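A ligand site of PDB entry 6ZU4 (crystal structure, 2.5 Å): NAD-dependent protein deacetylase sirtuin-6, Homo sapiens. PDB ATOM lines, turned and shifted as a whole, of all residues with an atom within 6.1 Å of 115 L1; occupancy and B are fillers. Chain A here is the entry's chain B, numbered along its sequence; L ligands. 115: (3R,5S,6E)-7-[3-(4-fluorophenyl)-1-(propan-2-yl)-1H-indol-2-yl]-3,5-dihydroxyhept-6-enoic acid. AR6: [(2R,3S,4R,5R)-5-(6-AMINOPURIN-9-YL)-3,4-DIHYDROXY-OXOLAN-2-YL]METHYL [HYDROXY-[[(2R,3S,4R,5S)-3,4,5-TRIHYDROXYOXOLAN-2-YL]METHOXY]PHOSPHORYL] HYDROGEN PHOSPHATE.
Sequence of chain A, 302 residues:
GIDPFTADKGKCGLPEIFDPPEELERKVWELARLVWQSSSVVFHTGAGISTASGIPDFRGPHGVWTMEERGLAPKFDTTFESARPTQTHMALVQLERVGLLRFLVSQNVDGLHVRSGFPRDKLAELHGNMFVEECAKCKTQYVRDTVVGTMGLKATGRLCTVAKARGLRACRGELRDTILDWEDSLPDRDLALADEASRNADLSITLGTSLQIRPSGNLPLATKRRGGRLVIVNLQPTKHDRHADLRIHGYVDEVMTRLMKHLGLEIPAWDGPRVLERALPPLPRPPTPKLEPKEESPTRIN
An oxygen (O1A) of 115 L1 is in hydrogen-bond range of the indole nitrogen (NE1) of Trp 182 (3.1 Å).
The side-chain amino group (NZ) of Lys 9 lies within salt-bridge range of an oxygen (O1A) of 115 L1, 3.3 Å away.
The backbone NH (N) of Phe 58 is in hydrogen-bond range of an oxygen (O2A) of AR6 L2, 2.6 Å away.
NE1 of Trp 65 is in hydrogen-bond range of O1D of AR6 L2, 3.4 Å away.
The side-chain amino group of Lys 9 lies within salt-bridge range of the side-chain carboxylate of Glu 68, 3.3 Å away.
N of Trp 65 sits at hydrogen-bond distance from O of Phe 58, 2.9 Å away.
O of Phe 58 sits at hydrogen-bond distance from N of Val 64 (3.3 Å).
O of Val 109 lies within hydrogen-bond range of N of Met 130, 2.9 Å away.
N of Val 64 sits at hydrogen-bond distance from O of Asp 57.
Residues that only touch 115 L1: Ile 55 (3.8 Å), Pro 56 (3.99 Å), Phe 58 (3.4 Å), Val 64 (3.7 Å), Trp 65 (3.4 Å), Glu 68 (3.6 Å), Pro 74 (3.5 Å), Phe 76 (3.3 Å), Phe 80 (3.7 Å), Val 109 (3.6 Å), Met 151 (3.4 Å) and Ile 179 (3.8 Å).
Hydrophobic or aromatic side chains that line 115 L1: Ile 55, Phe 58, Val 64, Trp 65, Pro 74, Phe 76, Phe 80, Val 109, Met 151, Ile 179 and Trp 182.
14 residues have an atom within 4 Å of 115 L1: Lys 9, Ile 55, Pro 56, Phe 58, Val 64, Trp 65, Glu 68, Pro 74, Phe 76, Phe 80, Val 109, Met 151, Ile 179 and Trp 182.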
ATOM      1  N   LYS A   9     -38.984  35.018  24.964  1.00  0.00           N
ATOM      2  CA  LYS A   9     -37.505  34.866  24.713  1.00  0.00           C
ATOM      3  C   LYS A   9     -36.689  35.626  25.771  1.00  0.00           C
ATOM      4  O   LYS A   9     -35.462  35.626  25.641  1.00  0.00           O
ATOM      5  CB  LYS A   9     -37.141  35.373  23.310  1.00  0.00           C
ATOM      6  CG  LYS A   9     -38.007  34.860  22.165  1.00  0.00           C
ATOM      7  CD  LYS A   9     -37.400  33.834  21.235  1.00  0.00           C
ATOM      8  CE  LYS A   9     -38.405  33.252  20.256  1.00  0.00           C
ATOM      9  NZ  LYS A   9     -37.827  33.077  18.904  1.00  0.00           N
ATOM     10  N   ILE A  55     -19.705  30.110  17.655  1.00  0.00           N
ATOM     11  CA  ILE A  55     -21.154  29.764  17.758  1.00  0.00           C
ATOM     12  C   ILE A  55     -21.827  30.868  18.562  1.00  0.00           C
ATOM     13  O   ILE A  55     -21.467  31.106  19.710  1.00  0.00           O
ATOM     14  CB  ILE A  55     -21.358  28.373  18.406  1.00  0.00           C
ATOM     15  CG1 ILE A  55     -20.565  27.291  17.680  1.00  0.00           C
ATOM     16  CG2 ILE A  55     -22.839  28.039  18.441  1.00  0.00           C
ATOM     17  CD1 ILE A  55     -20.808  25.928  18.214  1.00  0.00           C
ATOM     18  N   PRO A  56     -22.829  31.571  18.009  1.00  0.00           N
ATOM     19  CA  PRO A  56     -23.413  32.712  18.702  1.00  0.00           C
ATOM     20  C   PRO A  56     -24.305  32.224  19.857  1.00  0.00           C
ATOM     21  O   PRO A  56     -24.761  31.095  19.831  1.00  0.00           O
ATOM     22  CB  PRO A  56     -24.201  33.421  17.586  1.00  0.00           C
ATOM     23  CG  PRO A  56     -24.626  32.290  16.670  1.00  0.00           C
ATOM     24  CD  PRO A  56     -23.467  31.305  16.706  1.00  0.00           C
ATOM     25  N   ASP A  57     -24.495  33.096  20.853  1.00  0.00           N
ATOM     26  CA  ASP A  57     -25.388  32.823  22.007  1.00  0.00           C
ATOM     27  C   ASP A  57     -26.802  33.293  21.648  1.00  0.00           C
ATOM     28  O   ASP A  57     -27.093  33.362  20.448  1.00  0.00           O
ATOM     29  CB  ASP A  57     -24.824  33.416  23.297  1.00  0.00           C
ATOM     30  CG  ASP A  57     -24.649  34.910  23.244  1.00  0.00           C
ATOM     31  OD1 ASP A  57     -25.312  35.544  22.404  1.00  0.00           O
ATOM     32  OD2 ASP A  57     -23.826  35.409  24.033  1.00  0.00           O
ATOM     33  N   PHE A  58     -27.672  33.504  22.643  1.00  0.00           N
ATOM     34  CA  PHE A  58     -29.112  33.758  22.375  1.00  0.00           C
ATOM     35  C   PHE A  58     -29.435  35.219  22.707  1.00  0.00           C
ATOM     36  O   PHE A  58     -30.059  35.898  21.844  1.00  0.00           O
ATOM     37  CB  PHE A  58     -30.011  32.735  23.084  1.00  0.00           C
ATOM     38  CG  PHE A  58     -29.922  31.363  22.462  1.00  0.00           C
ATOM     39  CD1 PHE A  58     -30.551  31.081  21.265  1.00  0.00           C
ATOM     40  CD2 PHE A  58     -29.182  30.356  23.062  1.00  0.00           C
ATOM     41  CE1 PHE A  58     -30.461  29.824  20.688  1.00  0.00           C
ATOM     42  CE2 PHE A  58     -29.093  29.107  22.491  1.00  0.00           C
ATOM     43  CZ  PHE A  58     -29.718  28.846  21.299  1.00  0.00           C
ATOM     44  N   VAL A  64     -28.828  35.068  18.918  1.00  0.00           N
ATOM     45  CA  VAL A  64     -29.907  34.639  17.977  1.00  0.00           C
ATOM     46  C   VAL A  64     -31.138  35.544  18.183  1.00  0.00           C
ATOM     47  O   VAL A  64     -31.557  36.244  17.215  1.00  0.00           O
ATOM     48  CB  VAL A  64     -30.250  33.149  18.167  1.00  0.00           C
ATOM     49  CG1 VAL A  64     -31.396  32.718  17.266  1.00  0.00           C
ATOM     50  CG2 VAL A  64     -29.040  32.244  17.953  1.00  0.00           C
ATOM     51  N   TRP A  65     -31.663  35.566  19.414  1.00  0.00           N
ATOM     52  CA  TRP A  65     -32.913  36.261  19.799  1.00  0.00           C
ATOM     53  C   TRP A  65     -32.692  37.772  19.656  1.00  0.00           C
ATOM     54  O   TRP A  65     -33.549  38.445  19.042  1.00  0.00           O
ATOM     55  CB  TRP A  65     -33.379  35.865  21.204  1.00  0.00           C
ATOM     56  CG  TRP A  65     -33.661  34.412  21.467  1.00  0.00           C
ATOM     57  CD1 TRP A  65     -33.654  33.811  22.691  1.00  0.00           C
ATOM     58  CD2 TRP A  65     -33.950  33.363  20.516  1.00  0.00           C
ATOM     59  NE1 TRP A  65     -33.903  32.474  22.584  1.00  0.00           N
ATOM     60  CE2 TRP A  65     -34.103  32.158  21.262  1.00  0.00           C
ATOM     61  CE3 TRP A  65     -34.109  33.297  19.131  1.00  0.00           C
ATOM     62  CZ2 TRP A  65     -34.411  30.941  20.673  1.00  0.00           C
ATOM     63  CZ3 TRP A  65     -34.410  32.084  18.537  1.00  0.00           C
ATOM     64  CH2 TRP A  65     -34.562  30.918  19.298  1.00  0.00           C
ATOM     65  N   GLU A  68     -32.633  38.827  16.061  1.00  0.00           N
ATOM     66  CA  GLU A  68     -34.028  38.622  15.568  1.00  0.00           C
ATOM     67  C   GLU A  68     -34.871  39.875  15.868  1.00  0.00           C
ATOM     68  O   GLU A  68     -35.470  40.419  14.922  1.00  0.00           O
ATOM     69  CB  GLU A  68     -34.646  37.376  16.203  1.00  0.00           C
ATOM     70  CG  GLU A  68     -35.045  36.317  15.197  1.00  0.00           C
ATOM     71  CD  GLU A  68     -35.800  35.150  15.798  1.00  0.00           C
ATOM     72  OE1 GLU A  68     -36.456  35.327  16.853  1.00  0.00           O
ATOM     73  OE2 GLU A  68     -35.731  34.053  15.205  1.00  0.00           O
ATOM     74  N   PRO A  74     -28.109  36.072  13.200  1.00  0.00           N
ATOM     75  CA  PRO A  74     -26.971  35.648  13.997  1.00  0.00           C
ATOM     76  C   PRO A  74     -25.891  35.071  13.081  1.00  0.00           C
ATOM     77  O   PRO A  74     -26.239  34.442  12.125  1.00  0.00           O
ATOM     78  CB  PRO A  74     -27.590  34.569  14.901  1.00  0.00           C
ATOM     79  CG  PRO A  74     -28.627  33.925  13.992  1.00  0.00           C
ATOM     80  CD  PRO A  74     -29.235  35.120  13.282  1.00  0.00           C
ATOM     81  N   PHE A  76     -22.517  32.650  12.333  1.00  0.00           N
ATOM     82  CA  PHE A  76     -21.714  31.451  12.648  1.00  0.00           C
ATOM     83  C   PHE A  76     -20.352  31.597  11.975  1.00  0.00           C
ATOM     84  O   PHE A  76     -20.353  31.752  10.742  1.00  0.00           O
ATOM     85  CB  PHE A  76     -22.404  30.193  12.163  1.00  0.00           C
ATOM     86  CG  PHE A  76     -23.534  29.720  13.030  1.00  0.00           C
ATOM     87  CD1 PHE A  76     -24.821  30.211  12.849  1.00  0.00           C
ATOM     88  CD2 PHE A  76     -23.310  28.733  13.981  1.00  0.00           C
ATOM     89  CE1 PHE A  76     -25.851  29.772  13.653  1.00  0.00           C
ATOM     90  CE2 PHE A  76     -24.347  28.289  14.791  1.00  0.00           C
ATOM     91  CZ  PHE A  76     -25.606  28.831  14.632  1.00  0.00           C
ATOM     92  N   PHE A  80     -21.279  23.285  13.201  1.00  0.00           N
ATOM     93  CA  PHE A  80     -21.360  22.522  14.468  1.00  0.00           C
ATOM     94  C   PHE A  80     -20.356  21.369  14.402  1.00  0.00           C
ATOM     95  O   PHE A  80     -19.732  21.069  15.423  1.00  0.00           O
ATOM     96  CB  PHE A  80     -22.800  22.078  14.733  1.00  0.00           C
ATOM     97  CG  PHE A  80     -23.707  23.208  15.174  1.00  0.00           C
ATOM     98  CD1 PHE A  80     -23.561  23.796  16.423  1.00  0.00           C
ATOM     99  CD2 PHE A  80     -24.753  23.640  14.372  1.00  0.00           C
ATOM    100  CE1 PHE A  80     -24.420  24.790  16.846  1.00  0.00           C
ATOM    101  CE2 PHE A  80     -25.618  24.630  14.800  1.00  0.00           C
ATOM    102  CZ  PHE A  80     -25.436  25.225  16.029  1.00  0.00           C
ATOM    103  N   VAL A 109     -26.971  22.738  23.169  1.00  0.00           N
ATOM    104  CA  VAL A 109     -27.268  21.631  22.232  1.00  0.00           C
ATOM    105  C   VAL A 109     -26.103  21.461  21.242  1.00  0.00           C
ATOM    106  O   VAL A 109     -26.240  20.625  20.338  1.00  0.00           O
ATOM    107  CB  VAL A 109     -28.612  21.928  21.558  1.00  0.00           C
ATOM    108  CG1 VAL A 109     -29.730  21.997  22.593  1.00  0.00           C
ATOM    109  CG2 VAL A 109     -28.556  23.201  20.730  1.00  0.00           C
ATOM    110  N   ASP A 110     -25.002  22.184  21.443  1.00  0.00           N
ATOM    111  CA  ASP A 110     -23.905  22.355  20.440  1.00  0.00           C
ATOM    112  C   ASP A 110     -23.050  21.080  20.392  1.00  0.00           C
ATOM    113  O   ASP A 110     -22.233  20.961  19.463  1.00  0.00           O
ATOM    114  CB  ASP A 110     -23.033  23.586  20.732  1.00  0.00           C
ATOM    115  CG  ASP A 110     -22.452  23.641  22.147  1.00  0.00           C
ATOM    116  OD1 ASP A 110     -22.045  22.600  22.664  1.00  0.00           O
ATOM    117  OD2 ASP A 110     -22.439  24.758  22.752  1.00  0.00           O
ATOM    118  N   MET A 130     -27.482  18.095  19.474  1.00  0.00           N
ATOM    119  CA  MET A 130     -27.757  18.029  18.015  1.00  0.00           C
ATOM    120  C   MET A 130     -27.096  16.812  17.391  1.00  0.00           C
ATOM    121  O   MET A 130     -27.425  16.493  16.268  1.00  0.00           O
ATOM    122  CB  MET A 130     -27.232  19.296  17.337  1.00  0.00           C
ATOM    123  CG  MET A 130     -28.327  20.390  17.201  1.00  0.00           C
ATOM    124  SD  MET A 130     -27.695  21.886  16.397  1.00  0.00           S
ATOM    125  CE  MET A 130     -25.968  21.772  16.872  1.00  0.00           C
ATOM    126  N   MET A 151     -35.006  18.842  14.552  1.00  0.00           N
ATOM    127  CA  MET A 151     -35.121  19.455  15.894  1.00  0.00           C
ATOM    128  C   MET A 151     -36.574  19.303  16.357  1.00  0.00           C
ATOM    129  O   MET A 151     -37.432  19.145  15.488  1.00  0.00           O
ATOM    130  CB  MET A 151     -34.776  20.948  15.856  1.00  0.00           C
ATOM    131  CG  MET A 151     -33.312  21.244  15.548  1.00  0.00           C
ATOM    132  SD  MET A 151     -32.974  23.011  15.662  1.00  0.00           S
ATOM    133  CE  MET A 151     -34.330  23.665  14.676  1.00  0.00           C
ATOM    134  N   ILE A 179     -33.499  17.344  20.432  1.00  0.00           N
ATOM    135  CA  ILE A 179     -33.597  18.818  20.618  1.00  0.00           C
ATOM    136  C   ILE A 179     -35.029  19.153  21.032  1.00  0.00           C
ATOM    137  O   ILE A 179     -35.913  19.074  20.179  1.00  0.00           O
ATOM    138  CB  ILE A 179     -33.156  19.563  19.353  1.00  0.00           C
ATOM    139  CG1 ILE A 179     -31.786  19.077  18.897  1.00  0.00           C
ATOM    140  CG2 ILE A 179     -33.178  21.068  19.608  1.00  0.00           C
ATOM    141  CD1 ILE A 179     -30.693  19.432  19.885  1.00  0.00           C
ATOM    142  N   LEU A 180     -35.245  19.507  22.299  1.00  0.00           N
ATOM    143  CA  LEU A 180     -36.555  20.000  22.800  1.00  0.00           C
ATOM    144  C   LEU A 180     -36.995  21.224  21.998  1.00  0.00           C
ATOM    145  O   LEU A 180     -36.147  22.095  21.769  1.00  0.00           O
ATOM    146  CB  LEU A 180     -36.426  20.447  24.254  1.00  0.00           C
ATOM    147  CG  LEU A 180     -35.990  19.398  25.272  1.00  0.00           C
ATOM    148  CD1 LEU A 180     -35.901  20.027  26.631  1.00  0.00           C
ATOM    149  CD2 LEU A 180     -36.931  18.218  25.319  1.00  0.00           C
ATOM    150  N   ASP A 181     -38.286  21.309  21.682  1.00  0.00           N
ATOM    151  CA  ASP A 181     -38.972  22.558  21.247  1.00  0.00           C
ATOM    152  C   ASP A 181     -39.434  23.287  22.507  1.00  0.00           C
ATOM    153  O   ASP A 181     -39.389  22.651  23.569  1.00  0.00           O
ATOM    154  CB  ASP A 181     -40.161  22.228  20.343  1.00  0.00           C
ATOM    155  CG  ASP A 181     -40.495  23.312  19.336  1.00  0.00           C
ATOM    156  OD1 ASP A 181     -40.174  24.494  19.621  1.00  0.00           O
ATOM    157  OD2 ASP A 181     -41.054  22.966  18.265  1.00  0.00           O
ATOM    158  N   TRP A 182     -39.920  24.522  22.385  1.00  0.00           N
ATOM    159  CA  TRP A 182     -40.436  25.347  23.514  1.00  0.00           C
ATOM    160  C   TRP A 182     -41.366  24.541  24.440  1.00  0.00           C
ATOM    161  O   TRP A 182     -41.221  24.647  25.641  1.00  0.00           O
ATOM    162  CB  TRP A 182     -41.132  26.606  23.001  1.00  0.00           C
ATOM    163  CG  TRP A 182     -40.177  27.553  22.354  1.00  0.00           C
ATOM    164  CD1 TRP A 182     -39.948  27.711  21.012  1.00  0.00           C
ATOM    165  CD2 TRP A 182     -39.265  28.456  23.016  1.00  0.00           C
ATOM    166  NE1 TRP A 182     -38.992  28.660  20.805  1.00  0.00           N
ATOM    167  CE2 TRP A 182     -38.548  29.141  22.010  1.00  0.00           C
ATOM    168  CE3 TRP A 182     -39.002  28.769  24.361  1.00  0.00           C
ATOM    169  CZ2 TRP A 182     -37.588  30.100  22.308  1.00  0.00           C
ATOM    170  CZ3 TRP A 182     -38.054  29.718  24.653  1.00  0.00           C
ATOM    171  CH2 TRP A 182     -37.353  30.371  23.635  1.00  0.00           C
HETATM  172  C10 115 L   1     -28.717  27.695  17.264  1.00  0.00           C
HETATM  173  C15 115 L   1     -29.150  26.818  18.282  1.00  0.00           C
HETATM  174  C14 115 L   1     -28.314  26.462  19.340  1.00  0.00           C
HETATM  175  C13 115 L   1     -27.044  26.991  19.370  1.00  0.00           C
HETATM  176  C12 115 L   1     -26.598  27.863  18.382  1.00  0.00           C
HETATM  177  C11 115 L   1     -27.412  28.210  17.326  1.00  0.00           C
HETATM  178  C8  115 L   1     -29.793  27.847  16.348  1.00  0.00           C
HETATM  179  C9  115 L   1     -30.846  27.088  16.814  1.00  0.00           C
HETATM  180  N1  115 L   1     -30.451  26.442  17.998  1.00  0.00           N
HETATM  181  C83 115 L   1     -29.182  28.837  12.756  1.00  0.00           C
HETATM  182  C82 115 L   1     -29.279  28.085  13.922  1.00  0.00           C
HETATM  183  C81 115 L   1     -29.727  28.647  15.112  1.00  0.00           C
HETATM  184  C86 115 L   1     -30.079  29.990  15.105  1.00  0.00           C
HETATM  185  C85 115 L   1     -29.999  30.756  13.948  1.00  0.00           C
HETATM  186  C84 115 L   1     -29.535  30.159  12.802  1.00  0.00           C
HETATM  187  F1  115 L   1     -29.432  30.901  11.672  1.00  0.00           F
HETATM  188  O1B 115 L   1     -38.662  28.147  17.287  1.00  0.00           O
HETATM  189  O1A 115 L   1     -37.678  29.870  18.321  1.00  0.00           O
HETATM  190  O3  115 L   1     -35.370  30.438  14.941  1.00  0.00           O
HETATM  191  C1  115 L   1     -37.964  29.199  17.280  1.00  0.00           C
HETATM  192  C2  115 L   1     -37.409  29.683  15.952  1.00  0.00           C
HETATM  193  C3  115 L   1     -35.889  29.495  15.886  1.00  0.00           C
HETATM  194  C4  115 L   1     -35.462  28.082  15.509  1.00  0.00           C
HETATM  195  C5  115 L   1     -34.028  28.042  14.986  1.00  0.00           C
HETATM  196  C6  115 L   1     -33.013  27.919  16.087  1.00  0.00           C
HETATM  197  C7  115 L   1     -32.148  26.927  16.239  1.00  0.00           C
HETATM  198  C91 115 L   1     -31.200  25.569  18.913  1.00  0.00           C
HETATM  199  C92 115 L   1     -31.343  24.179  18.365  1.00  0.00           C
HETATM  200  C93 115 L   1     -32.510  26.177  19.402  1.00  0.00           C
HETATM  201  O5  115 L   1     -33.927  26.940  14.065  1.00  0.00           O
HETATM  202  N1  AR6 L   2     -17.669  34.970  28.370  1.00  0.00           N
HETATM  203  C2  AR6 L   2     -18.611  35.164  29.314  1.00  0.00           C
HETATM  204  N3  AR6 L   2     -19.922  35.284  29.186  1.00  0.00           N
HETATM  205  C4  AR6 L   2     -20.262  35.194  27.881  1.00  0.00           C
HETATM  206  C5  AR6 L   2     -19.407  35.026  26.813  1.00  0.00           C
HETATM  207  C6  AR6 L   2     -18.042  34.902  27.078  1.00  0.00           C
HETATM  208  N6  AR6 L   2     -17.125  34.704  26.115  1.00  0.00           N
HETATM  209  N7  AR6 L   2     -20.125  35.018  25.628  1.00  0.00           N
HETATM  210  C8  AR6 L   2     -21.378  35.172  26.002  1.00  0.00           C
HETATM  211  N9  AR6 L   2     -21.510  35.295  27.342  1.00  0.00           N
HETATM  212  PA  AR6 L   2     -28.055  33.057  26.658  1.00  0.00           P
HETATM  213  PB  AR6 L   2     -28.307  30.435  27.761  1.00  0.00           P
HETATM  214  C1' AR6 L   2     -22.758  35.432  28.072  1.00  0.00           C
HETATM  215  O1A AR6 L   2     -29.391  33.205  27.304  1.00  0.00           O
HETATM  216  O1B AR6 L   2     -27.552  29.157  27.514  1.00  0.00           O
HETATM  217  C1D AR6 L   2     -32.491  29.523  24.720  1.00  0.00           C
HETATM  218  O1D AR6 L   2     -33.814  29.559  24.359  1.00  0.00           O
HETATM  219  C2' AR6 L   2     -23.742  36.480  27.582  1.00  0.00           C
HETATM  220  O2' AR6 L   2     -23.476  37.723  28.212  1.00  0.00           O
HETATM  221  O2A AR6 L   2     -27.770  33.466  25.254  1.00  0.00           O
HETATM  222  O2B AR6 L   2     -28.250  31.091  29.104  1.00  0.00           O
HETATM  223  C2D AR6 L   2     -31.993  28.113  24.436  1.00  0.00           C
HETATM  224  O2D AR6 L   2     -32.957  27.148  24.782  1.00  0.00           O
HETATM  225  C3' AR6 L   2     -25.113  35.881  27.984  1.00  0.00           C
HETATM  226  O3' AR6 L   2     -25.812  36.369  29.140  1.00  0.00           O
HETATM  227  O3A AR6 L   2     -27.687  31.503  26.760  1.00  0.00           O
HETATM  228  C3D AR6 L   2     -30.870  27.945  25.432  1.00  0.00           C
HETATM  229  O3D AR6 L   2     -30.640  26.547  25.548  1.00  0.00           O
HETATM  230  C4' AR6 L   2     -24.821  34.391  28.209  1.00  0.00           C
HETATM  231  O4' AR6 L   2     -23.407  34.197  27.949  1.00  0.00           O
HETATM  232  C4D AR6 L   2     -31.507  28.608  26.671  1.00  0.00           C
HETATM  233  O4D AR6 L   2     -32.327  29.687  26.141  1.00  0.00           O
HETATM  234  C5' AR6 L   2     -25.607  33.477  27.314  1.00  0.00           C
HETATM  235  O5' AR6 L   2     -26.987  33.712  27.615  1.00  0.00           O
HETATM  236  C5D AR6 L   2     -30.572  29.129  27.746  1.00  0.00           C
HETATM  237  O5D AR6 L   2     -29.807  30.264  27.257  1.00  0.00           O
